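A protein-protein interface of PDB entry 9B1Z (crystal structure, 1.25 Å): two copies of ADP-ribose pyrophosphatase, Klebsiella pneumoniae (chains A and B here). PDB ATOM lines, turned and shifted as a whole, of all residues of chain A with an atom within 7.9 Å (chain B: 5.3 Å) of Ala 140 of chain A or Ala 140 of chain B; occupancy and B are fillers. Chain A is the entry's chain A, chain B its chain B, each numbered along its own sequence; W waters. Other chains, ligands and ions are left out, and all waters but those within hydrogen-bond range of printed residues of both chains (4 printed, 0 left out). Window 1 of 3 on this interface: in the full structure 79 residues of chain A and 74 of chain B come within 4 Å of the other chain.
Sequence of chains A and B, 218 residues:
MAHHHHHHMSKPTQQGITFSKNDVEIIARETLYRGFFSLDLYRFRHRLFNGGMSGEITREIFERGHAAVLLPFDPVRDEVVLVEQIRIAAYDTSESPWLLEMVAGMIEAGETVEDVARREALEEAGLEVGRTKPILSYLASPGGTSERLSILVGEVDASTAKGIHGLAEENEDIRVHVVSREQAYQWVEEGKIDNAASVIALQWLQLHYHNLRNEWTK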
ATOM      1  N   ARG A  64      17.277  26.954  15.135  1.00  0.00           N
ATOM      2  CA  ARG A  64      18.020  25.762  14.743  1.00  0.00           C
ATOM      3  C   ARG A  64      19.458  26.100  14.364  1.00  0.00           C
ATOM      4  O   ARG A  64      20.107  25.317  13.659  1.00  0.00           O
ATOM      5  CB  ARG A  64      17.324  25.042  13.593  1.00  0.00           C
ATOM      6  CG  ARG A  64      17.146  25.926  12.374  1.00  0.00           C
ATOM      7  CD  ARG A  64      16.970  25.097  11.125  1.00  0.00           C
ATOM      8  NE  ARG A  64      18.132  24.246  10.914  1.00  0.00           N
ATOM      9  CZ  ARG A  64      18.175  23.247  10.053  1.00  0.00           C
ATOM     10  NH1 ARG A  64      17.119  22.912   9.336  1.00  0.00           N
ATOM     11  NH2 ARG A  64      19.312  22.576   9.896  1.00  0.00           N
ATOM     12  N   SER A 137      24.018  35.783   1.546  1.00  0.00           N
ATOM     13  CA  SER A 137      23.622  35.262   2.842  1.00  0.00           C
ATOM     14  C   SER A 137      22.199  35.711   3.100  1.00  0.00           C
ATOM     15  O   SER A 137      21.912  36.904   2.998  1.00  0.00           O
ATOM     16  CB  SER A 137      24.550  35.790   3.933  1.00  0.00           C
ATOM     17  OG  SER A 137      24.126  35.369   5.215  1.00  0.00           O
ATOM     18  N   TYR A 138      21.312  34.767   3.418  1.00  0.00           N
ATOM     19  CA  TYR A 138      19.886  35.062   3.475  1.00  0.00           C
ATOM     20  C   TYR A 138      19.229  34.447   4.704  1.00  0.00           C
ATOM     21  O   TYR A 138      19.663  33.430   5.244  1.00  0.00           O
ATOM     22  CB  TYR A 138      19.143  34.585   2.199  1.00  0.00           C
ATOM     23  CG  TYR A 138      19.040  33.076   2.074  1.00  0.00           C
ATOM     24  CD1 TYR A 138      20.092  32.318   1.564  1.00  0.00           C
ATOM     25  CD2 TYR A 138      17.897  32.406   2.450  1.00  0.00           C
ATOM     26  CE1 TYR A 138      20.015  30.969   1.495  1.00  0.00           C
ATOM     27  CE2 TYR A 138      17.802  31.036   2.354  1.00  0.00           C
ATOM     28  CZ  TYR A 138      18.865  30.324   1.879  1.00  0.00           C
ATOM     29  OH  TYR A 138      18.823  28.953   1.792  1.00  0.00           O
ATOM     30  N   LEU A 139      18.132  35.073   5.109  1.00  0.00           N
ATOM     31  CA  LEU A 139      17.227  34.573   6.134  1.00  0.00           C
ATOM     32  C   LEU A 139      16.180  33.695   5.453  1.00  0.00           C
ATOM     33  O   LEU A 139      15.485  34.146   4.535  1.00  0.00           O
ATOM     34  CB  LEU A 139      16.562  35.751   6.836  1.00  0.00           C
ATOM     35  CG  LEU A 139      17.512  36.615   7.660  1.00  0.00           C
ATOM     36  CD1 LEU A 139      16.901  37.986   7.894  1.00  0.00           C
ATOM     37  CD2 LEU A 139      17.828  35.931   8.982  1.00  0.00           C
ATOM     38  N   ALA A 140      16.089  32.431   5.875  1.00  0.00           N
ATOM     39  CA  ALA A 140      15.216  31.473   5.200  1.00  0.00           C
ATOM     40  C   ALA A 140      13.750  31.885   5.241  1.00  0.00           C
ATOM     41  O   ALA A 140      13.024  31.701   4.254  1.00  0.00           O
ATOM     42  CB  ALA A 140      15.384  30.083   5.826  1.00  0.00           C
ATOM     43  N   SER A 141      13.272  32.351   6.399  1.00  0.00           N
ATOM     44  CA  SER A 141      11.858  32.661   6.573  1.00  0.00           C
ATOM     45  C   SER A 141      11.713  33.470   7.854  1.00  0.00           C
ATOM     46  O   SER A 141      11.318  32.936   8.899  1.00  0.00           O
ATOM     47  CB  SER A 141      11.016  31.393   6.630  1.00  0.00           C
ATOM     48  OG  SER A 141       9.659  31.747   6.717  1.00  0.00           O
ATOM     49  N   PRO A 142      12.040  34.759   7.814  1.00  0.00           N
ATOM     50  CA  PRO A 142      12.244  35.500   9.059  1.00  0.00           C
ATOM     51  C   PRO A 142      10.976  35.860   9.809  1.00  0.00           C
ATOM     52  O   PRO A 142      11.085  36.427  10.894  1.00  0.00           O
ATOM     53  CB  PRO A 142      13.007  36.749   8.599  1.00  0.00           C
ATOM     54  CG  PRO A 142      12.642  36.908   7.169  1.00  0.00           C
ATOM     55  CD  PRO A 142      12.499  35.513   6.640  1.00  0.00           C
ATOM     56  N   GLY A 143       9.792  35.543   9.287  1.00  0.00           N
ATOM     57  CA  GLY A 143       8.578  35.680  10.063  1.00  0.00           C
ATOM     58  C   GLY A 143       8.398  34.614  11.124  1.00  0.00           C
ATOM     59  O   GLY A 143       7.561  34.791  12.011  1.00  0.00           O
ATOM     60  N   GLY A 144       9.179  33.539  11.083  1.00  0.00           N
ATOM     61  CA  GLY A 144       9.017  32.467  12.042  1.00  0.00           C
ATOM     62  C   GLY A 144      10.263  31.708  12.433  1.00  0.00           C
ATOM     63  O   GLY A 144      10.172  30.882  13.339  1.00  0.00           O
ATOM     64  N   THR A 145      11.406  31.936  11.779  1.00  0.00           N
ATOM     65  CA  THR A 145      12.647  31.265  12.152  1.00  0.00           C
ATOM     66  C   THR A 145      13.812  32.243  12.059  1.00  0.00           C
ATOM     67  O   THR A 145      13.830  33.129  11.195  1.00  0.00           O
ATOM     68  CB  THR A 145      12.911  30.001  11.306  1.00  0.00           C
ATOM     69  OG1 THR A 145      14.115  29.358  11.742  1.00  0.00           O
ATOM     70  CG2 THR A 145      13.049  30.308   9.840  1.00  0.00           C
ATOM     71  N   SER A 146      14.779  32.096  12.964  1.00  0.00           N
ATOM     72  CA  SER A 146      15.965  32.937  12.926  1.00  0.00           C
ATOM     73  C   SER A 146      16.990  32.488  11.891  1.00  0.00           C
ATOM     74  O   SER A 146      17.993  33.188  11.693  1.00  0.00           O
ATOM     75  CB  SER A 146      16.638  32.913  14.286  1.00  0.00           C
ATOM     76  OG  SER A 146      17.001  31.583  14.587  1.00  0.00           O
ATOM     77  N   GLU A 147      16.772  31.351  11.241  1.00  0.00           N
ATOM     78  CA  GLU A 147      17.827  30.722  10.463  1.00  0.00           C
ATOM     79  C   GLU A 147      18.354  31.623   9.356  1.00  0.00           C
ATOM     80  O   GLU A 147      17.600  32.106   8.498  1.00  0.00           O
ATOM     81  CB  GLU A 147      17.326  29.417   9.852  1.00  0.00           C
ATOM     82  CG  GLU A 147      18.451  28.627   9.201  1.00  0.00           C
ATOM     83  CD  GLU A 147      17.998  27.381   8.494  1.00  0.00           C
ATOM     84  OE1 GLU A 147      16.806  27.314   8.106  1.00  0.00           O
ATOM     85  OE2 GLU A 147      18.854  26.491   8.281  1.00  0.00           O
ATOM     86  N   ARG A 148      19.680  31.763   9.337  1.00  0.00           N
ATOM     87  CA  ARG A 148      20.424  32.381   8.251  1.00  0.00           C
ATOM     88  C   ARG A 148      21.303  31.321   7.592  1.00  0.00           C
ATOM     89  O   ARG A 148      21.874  30.465   8.274  1.00  0.00           O
ATOM     90  CB  ARG A 148      21.302  33.513   8.798  1.00  0.00           C
ATOM     91  CG  ARG A 148      22.183  34.173   7.757  1.00  0.00           C
ATOM     92  CD  ARG A 148      22.853  35.438   8.303  1.00  0.00           C
ATOM     93  NE  ARG A 148      21.920  36.548   8.486  1.00  0.00           N
ATOM     94  CZ  ARG A 148      21.552  37.380   7.522  1.00  0.00           C
ATOM     95  NH1 ARG A 148      21.966  37.227   6.274  1.00  0.00           N
ATOM     96  NH2 ARG A 148      20.726  38.385   7.807  1.00  0.00           N
ATOM     97  N   LEU A 149      21.418  31.396   6.269  1.00  0.00           N
ATOM     98  CA  LEU A 149      22.240  30.502   5.466  1.00  0.00           C
ATOM     99  C   LEU A 149      23.124  31.357   4.579  1.00  0.00           C
ATOM    100  O   LEU A 149      22.646  32.279   3.909  1.00  0.00           O
ATOM    101  CB  LEU A 149      21.373  29.582   4.609  1.00  0.00           C
ATOM    102  CG  LEU A 149      20.426  28.681   5.404  1.00  0.00           C
ATOM    103  CD1 LEU A 149      19.057  29.322   5.557  1.00  0.00           C
ATOM    104  CD2 LEU A 149      20.277  27.303   4.770  1.00  0.00           C
ATOM    105  N   ASP A 194      13.534  23.049  -5.941  1.00  0.00           N
ATOM    106  CA  ASP A 194      12.612  24.042  -5.396  1.00  0.00           C
ATOM    107  C   ASP A 194      12.815  24.263  -3.904  1.00  0.00           C
ATOM    108  O   ASP A 194      11.851  24.536  -3.190  1.00  0.00           O
ATOM    109  CB  ASP A 194      11.143  23.760  -5.751  1.00  0.00           C
ATOM    110  CG  ASP A 194      10.546  22.586  -5.004  1.00  0.00           C
ATOM    111  OD1 ASP A 194      11.283  21.781  -4.396  1.00  0.00           O
ATOM    112  OD2 ASP A 194       9.306  22.472  -5.054  1.00  0.00           O
ATOM    113  N   ASN A 195      14.046  24.150  -3.421  1.00  0.00           N
ATOM    114  CA  ASN A 195      14.408  24.531  -2.065  1.00  0.00           C
ATOM    115  C   ASN A 195      15.194  25.834  -2.150  1.00  0.00           C
ATOM    116  O   ASN A 195      15.957  26.043  -3.099  1.00  0.00           O
ATOM    117  CB  ASN A 195      15.196  23.418  -1.365  1.00  0.00           C
ATOM    118  CG  ASN A 195      16.431  22.996  -2.135  1.00  0.00           C
ATOM    119  OD1 ASN A 195      17.527  23.500  -1.888  1.00  0.00           O
ATOM    120  ND2 ASN A 195      16.262  22.069  -3.081  1.00  0.00           N
ATOM    121  N   ALA A 196      14.977  26.718  -1.167  1.00  0.00           N
ATOM    122  CA  ALA A 196      15.493  28.083  -1.259  1.00  0.00           C
ATOM    123  C   ALA A 196      16.985  28.131  -1.567  1.00  0.00           C
ATOM    124  O   ALA A 196      17.418  28.900  -2.427  1.00  0.00           O
ATOM    125  CB  ALA A 196      15.212  28.846   0.026  1.00  0.00           C
ATOM    126  N   ALA A 197      17.796  27.356  -0.845  1.00  0.00           N
ATOM    127  CA  ALA A 197      19.235  27.493  -1.000  1.00  0.00           C
ATOM    128  C   ALA A 197      19.656  27.201  -2.434  1.00  0.00           C
ATOM    129  O   ALA A 197      20.514  27.895  -2.996  1.00  0.00           O
ATOM    130  CB  ALA A 197      19.970  26.539  -0.053  1.00  0.00           C
ATOM    131  N   ILE A 200      18.291  29.962  -4.964  1.00  0.00           N
ATOM    132  CA  ILE A 200      19.086  31.191  -4.885  1.00  0.00           C
ATOM    133  C   ILE A 200      20.444  30.973  -5.537  1.00  0.00           C
ATOM    134  O   ILE A 200      20.913  31.807  -6.314  1.00  0.00           O
ATOM    135  CB  ILE A 200      19.216  31.657  -3.423  1.00  0.00           C
ATOM    136  CG1 ILE A 200      17.851  32.125  -2.917  1.00  0.00           C
ATOM    137  CG2 ILE A 200      20.255  32.736  -3.298  1.00  0.00           C
ATOM    138  CD1 ILE A 200      17.777  32.395  -1.434  1.00  0.00           C
ATOM    139  N   TYR B 138       8.770  27.536  -3.518  1.00  0.00           N
ATOM    140  CA  TYR B 138       9.953  26.972  -2.892  1.00  0.00           C
ATOM    141  C   TYR B 138       9.707  26.587  -1.443  1.00  0.00           C
ATOM    142  O   TYR B 138       8.868  27.160  -0.755  1.00  0.00           O
ATOM    143  CB  TYR B 138      11.157  27.926  -2.985  1.00  0.00           C
ATOM    144  CG  TYR B 138      11.023  29.158  -2.126  1.00  0.00           C
ATOM    145  CD1 TYR B 138      10.311  30.273  -2.567  1.00  0.00           C
ATOM    146  CD2 TYR B 138      11.570  29.210  -0.854  1.00  0.00           C
ATOM    147  CE1 TYR B 138      10.152  31.382  -1.758  1.00  0.00           C
ATOM    148  CE2 TYR B 138      11.423  30.327  -0.049  1.00  0.00           C
ATOM    149  CZ  TYR B 138      10.715  31.400  -0.515  1.00  0.00           C
ATOM    150  OH  TYR B 138      10.523  32.510   0.256  1.00  0.00           O
ATOM    151  N   LEU B 139      10.476  25.607  -0.995  1.00  0.00           N
ATOM    152  CA  LEU B 139      10.567  25.221   0.400  1.00  0.00           C
ATOM    153  C   LEU B 139      11.605  26.103   1.086  1.00  0.00           C
ATOM    154  O   LEU B 139      12.761  26.168   0.656  1.00  0.00           O
ATOM    155  CB  LEU B 139      10.999  23.758   0.468  1.00  0.00           C
ATOM    156  CG  LEU B 139       9.973  22.769  -0.088  1.00  0.00           C
ATOM    157  CD1 LEU B 139      10.655  21.462  -0.483  1.00  0.00           C
ATOM    158  CD2 LEU B 139       8.856  22.545   0.914  1.00  0.00           C
ATOM    159  N   ALA B 140      11.192  26.788   2.150  1.00  0.00           N
ATOM    160  CA  ALA B 140      12.070  27.742   2.819  1.00  0.00           C
ATOM    161  C   ALA B 140      13.321  27.094   3.385  1.00  0.00           C
ATOM    162  O   ALA B 140      14.406  27.664   3.288  1.00  0.00           O
ATOM    163  CB  ALA B 140      11.330  28.462   3.943  1.00  0.00           C
ATOM    164  N   SER B 141      13.174  25.945   4.036  1.00  0.00           N
ATOM    165  CA  SER B 141      14.282  25.294   4.730  1.00  0.00           C
ATOM    166  C   SER B 141      13.860  23.882   5.100  1.00  0.00           C
ATOM    167  O   SER B 141      13.519  23.603   6.260  1.00  0.00           O
ATOM    168  CB  SER B 141      14.691  26.076   5.967  1.00  0.00           C
ATOM    169  OG  SER B 141      15.830  25.474   6.546  1.00  0.00           O
ATOM    170  N   PRO B 142      13.846  22.973   4.129  1.00  0.00           N
ATOM    171  CA  PRO B 142      13.152  21.695   4.321  1.00  0.00           C
ATOM    172  C   PRO B 142      13.842  20.716   5.253  1.00  0.00           C
ATOM    173  O   PRO B 142      13.260  19.677   5.542  1.00  0.00           O
ATOM    174  CB  PRO B 142      13.016  21.170   2.895  1.00  0.00           C
ATOM    175  CG  PRO B 142      14.161  21.789   2.150  1.00  0.00           C
ATOM    176  CD  PRO B 142      14.317  23.157   2.750  1.00  0.00           C
ATOM    177  N   THR B 145      11.619  22.672   8.510  1.00  0.00           N
ATOM    178  CA  THR B 145      10.265  23.204   8.424  1.00  0.00           C
ATOM    179  C   THR B 145       9.610  22.741   7.130  1.00  0.00           C
ATOM    180  O   THR B 145      10.271  22.585   6.101  1.00  0.00           O
ATOM    181  CB  THR B 145      10.245  24.759   8.533  1.00  0.00           C
ATOM    182  OG1 THR B 145       8.900  25.238   8.488  1.00  0.00           O
ATOM    183  CG2 THR B 145      11.015  25.434   7.415  1.00  0.00           C
ATOM    184  N   GLU B 147       7.498  24.578   5.556  1.00  0.00           N
ATOM    185  CA  GLU B 147       6.940  25.754   4.912  1.00  0.00           C
ATOM    186  C   GLU B 147       7.308  25.859   3.442  1.00  0.00           C
ATOM    187  O   GLU B 147       8.489  25.821   3.065  1.00  0.00           O
ATOM    188  CB  GLU B 147       7.404  27.013   5.627  1.00  0.00           C
ATOM    189  CG  GLU B 147       6.706  28.248   5.098  1.00  0.00           C
ATOM    190  CD  GLU B 147       7.221  29.562   5.667  1.00  0.00           C
ATOM    191  OE1 GLU B 147       8.387  29.596   6.116  1.00  0.00           O
ATOM    192  OE2 GLU B 147       6.480  30.563   5.608  1.00  0.00           O
ATOM    193  N   ARG B 148       6.277  26.044   2.637  1.00  0.00           N
ATOM    194  CA  ARG B 148       6.386  26.351   1.222  1.00  0.00           C
ATOM    195  C   ARG B 148       5.829  27.749   0.986  1.00  0.00           C
ATOM    196  O   ARG B 148       4.831  28.143   1.602  1.00  0.00           O
ATOM    197  CB  ARG B 148       5.607  25.321   0.401  1.00  0.00           C
ATOM    198  CG  ARG B 148       5.585  25.605  -1.091  1.00  0.00           C
ATOM    199  CD  ARG B 148       5.030  24.439  -1.890  1.00  0.00           C
ATOM    200  NE  ARG B 148       5.942  23.297  -1.923  1.00  0.00           N
ATOM    201  CZ  ARG B 148       6.938  23.153  -2.785  1.00  0.00           C
ATOM    202  NH1 ARG B 148       7.218  24.084  -3.675  1.00  0.00           N
ATOM    203  NH2 ARG B 148       7.648  22.026  -2.775  1.00  0.00           N
ATOM    204  N   LEU B 149       6.498  28.505   0.116  1.00  0.00           N
ATOM    205  CA  LEU B 149       6.089  29.845  -0.275  1.00  0.00           C
ATOM    206  C   LEU B 149       6.003  29.879  -1.792  1.00  0.00           C
ATOM    207  O   LEU B 149       6.940  29.472  -2.485  1.00  0.00           O
ATOM    208  CB  LEU B 149       7.073  30.905   0.237  1.00  0.00           C
ATOM    209  CG  LEU B 149       7.247  30.944   1.761  1.00  0.00           C
ATOM    210  CD1 LEU B 149       8.410  30.082   2.210  1.00  0.00           C
ATOM    211  CD2 LEU B 149       7.442  32.365   2.254  1.00  0.00           C
ATOM    212  N   ALA B 196      14.813  35.219   1.886  1.00  0.00           N
ATOM    213  CA  ALA B 196      14.711  34.310   0.749  1.00  0.00           C
ATOM    214  C   ALA B 196      13.670  34.746  -0.269  1.00  0.00           C
ATOM    215  O   ALA B 196      13.930  34.715  -1.470  1.00  0.00           O
ATOM    216  CB  ALA B 196      14.399  32.896   1.223  1.00  0.00           C
HETATM  217  O   HOH W   1       9.798  19.594  -3.786  1.00  0.00           O
HETATM  218  O   HOH W   2      14.592  24.459   9.026  1.00  0.00           O
HETATM  219  O   HOH W   3      17.001  27.255   2.863  1.00  0.00           O
HETATM  220  O   HOH W   4      11.180  32.940   2.794  1.00  0.00           O
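N of Ala 196 of chain A lies within hydrogen-bond range of O of Leu 139 of chain B (2.9 Å).
O of Leu 139 of chain A sits at hydrogen-bond distance from N of Ala 196 of chain B, at 2.9 Å.
NH2 of Arg 148 of chain B lies within salt-bridge range of OD2 of Asp 194 of chain A, 2.9 Å away.
OG of Ser 141 of chain A sits at hydrogen-bond distance from OE1 of Glu 147 of chain B (2.6 Å).
N of Leu 139 of chain B lies within hydrogen-bond range of O of Asp 194 of chain A, at 2.8 Å.
OE1 of Glu 147 of chain A sits at hydrogen-bond distance from OG of Ser 141 of chain B, at 2.6 Å.
The backbone NH (N) of Ala 140 of chain A is in hydrogen-bond range of the backbone carbonyl oxygen (O) of Glu 147 of chain A (3.0 Å).
The backbone NH (N) of Tyr 138 of chain A is in hydrogen-bond range of the backbone carbonyl oxygen (O) of Leu 149 of chain A, at 2.9 Å.
The backbone NH of Glu 147 of chain A lies close to the side-chain hydroxyl of Thr 145 of chain A.
O of Leu 149 of chain B lies within hydrogen-bond range of N of Tyr 138 of chain B, 2.9 Å away.
The backbone NH (N) of Glu 147 of chain B lies close to the side-chain hydroxyl (OG1) of Thr 145 of chain B (3.3 Å).
The backbone carbonyl oxygen (O) of Glu 147 of chain B sits at hydrogen-bond distance from the backbone NH (N) of Ala 140 of chain B, 3.0 Å away.
Among the printed residues, merely in contact across the chains: Asp 194 of chain A with Tyr 138 of chain B (3.1 Å), Ala 140 of chain A with Ala 196 of chain B (3.5 Å), Ala 196 of chain A with Ala 140 of chain B (3.6 Å), Asn 195 of chain A with Leu 139 of chain B (3.6 Å), Ala 140 of chain A with Ala 140 of chain B (3.6 Å), Tyr 138 of chain A with Ala 196 of chain B (3.7 Å), Ala 196 of chain A with Tyr 138 of chain B (3.8 Å) and Ser 141 of chain A with Ala 140 of chain B (3.99 Å).
Printed residues of chain B within 4 Å of Tyr 138 of chain A: Ala 196 (3.7 Å).
Ala 140 of chain A touches just these residues of chain B: Ala 140 (3.6 Å) and Ala 196 (3.5 Å).
Pro 142 of chain A touches none of the printed residues of chain B.
Of the printed residues of chain B, Glu 147 of chain A touches Ser 141.
Arg 148 of chain A touches none of the printed residues of chain B.
Of the printed residues of chain B, Ala 196 of chain A touches Tyr 138 (3.8 Å), Leu 139 (2.9 Å) and Ala 140 (3.6 Å).
Printed residues of chain A within 4 Å of Ala 140 of chain B: Ala 140, Ser 141 and Ala 196.
Printed residues of chain A within 4 Å of Glu 147 of chain B: Ser 141.
Of the printed residues of chain A, Arg 148 of chain B touches Asp 194.
The nearest residue of chain B that does not touch Ala 140 of chain A is Ser 141 of chain B (4.1 Å).
The nearest printed residue of chain A that does not touch Ala 140 of chain B is Tyr 138 of chain A (4.8 Å).
The nearest printed residue of chain A that does not touch Glu 147 of chain B is Ala 140 of chain A (5.4 Å).
Of the 10 printed residues of chain B, 7 touch a printed residue of chain A.
Hydrophobic or aromatic side chains of chain B that line the printed part of chain A: Tyr 138, Leu 139, Ala 140 and Ala 196.
Among the printed residues, Asp or Glu carboxylates within 4 Å of a Lys or Arg side-chain nitrogen of the other chain: Asp 194 of chain A with Arg 148 of chain B (2.9 Å).
Leu 139 of chain A touches Ala 196 of chain B, and with the chains exchanged Ala 196 of chain A touches Leu 139 of chain B.
Ala 140 of chain A touches Ala 196 of chain B, and with the chains exchanged Ala 196 of chain A touches Ala 140 of chain B.
Ser 141 of chain A touches Ala 140 of chain B, but with the chains exchanged Ala 140 of chain A does not touch Ser 141 of chain B (4.1 Å).
Ser 141 of chain A touches Glu 147 of chain B, and with the chains exchanged Glu 147 of chain A touches Ser 141 of chain B.
10 positions are printed for both chains.
Of the 14 pairs that touch across the chains among the printed residues, 9 have their exchanged pair printed and touching as well.
Water W4 bridges OH of Tyr 138 of chain B (2.7 Å) and O of Ala 140 of chain A (2.7 Å).
Water W3 lies within hydrogen-bond range of O of Ala 140 of chain B (2.7 Å) and OH of Tyr 138 of chain A (2.7 Å).
Water W1 bridges OD1 of Asp 194 of chain A (2.7 Å) and NH2 of Arg 148 of chain B (3.4 Å).
Water W2 lies within hydrogen-bond range of OG of Ser 141 of chain B and NH1 of Arg 64 of chain A.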
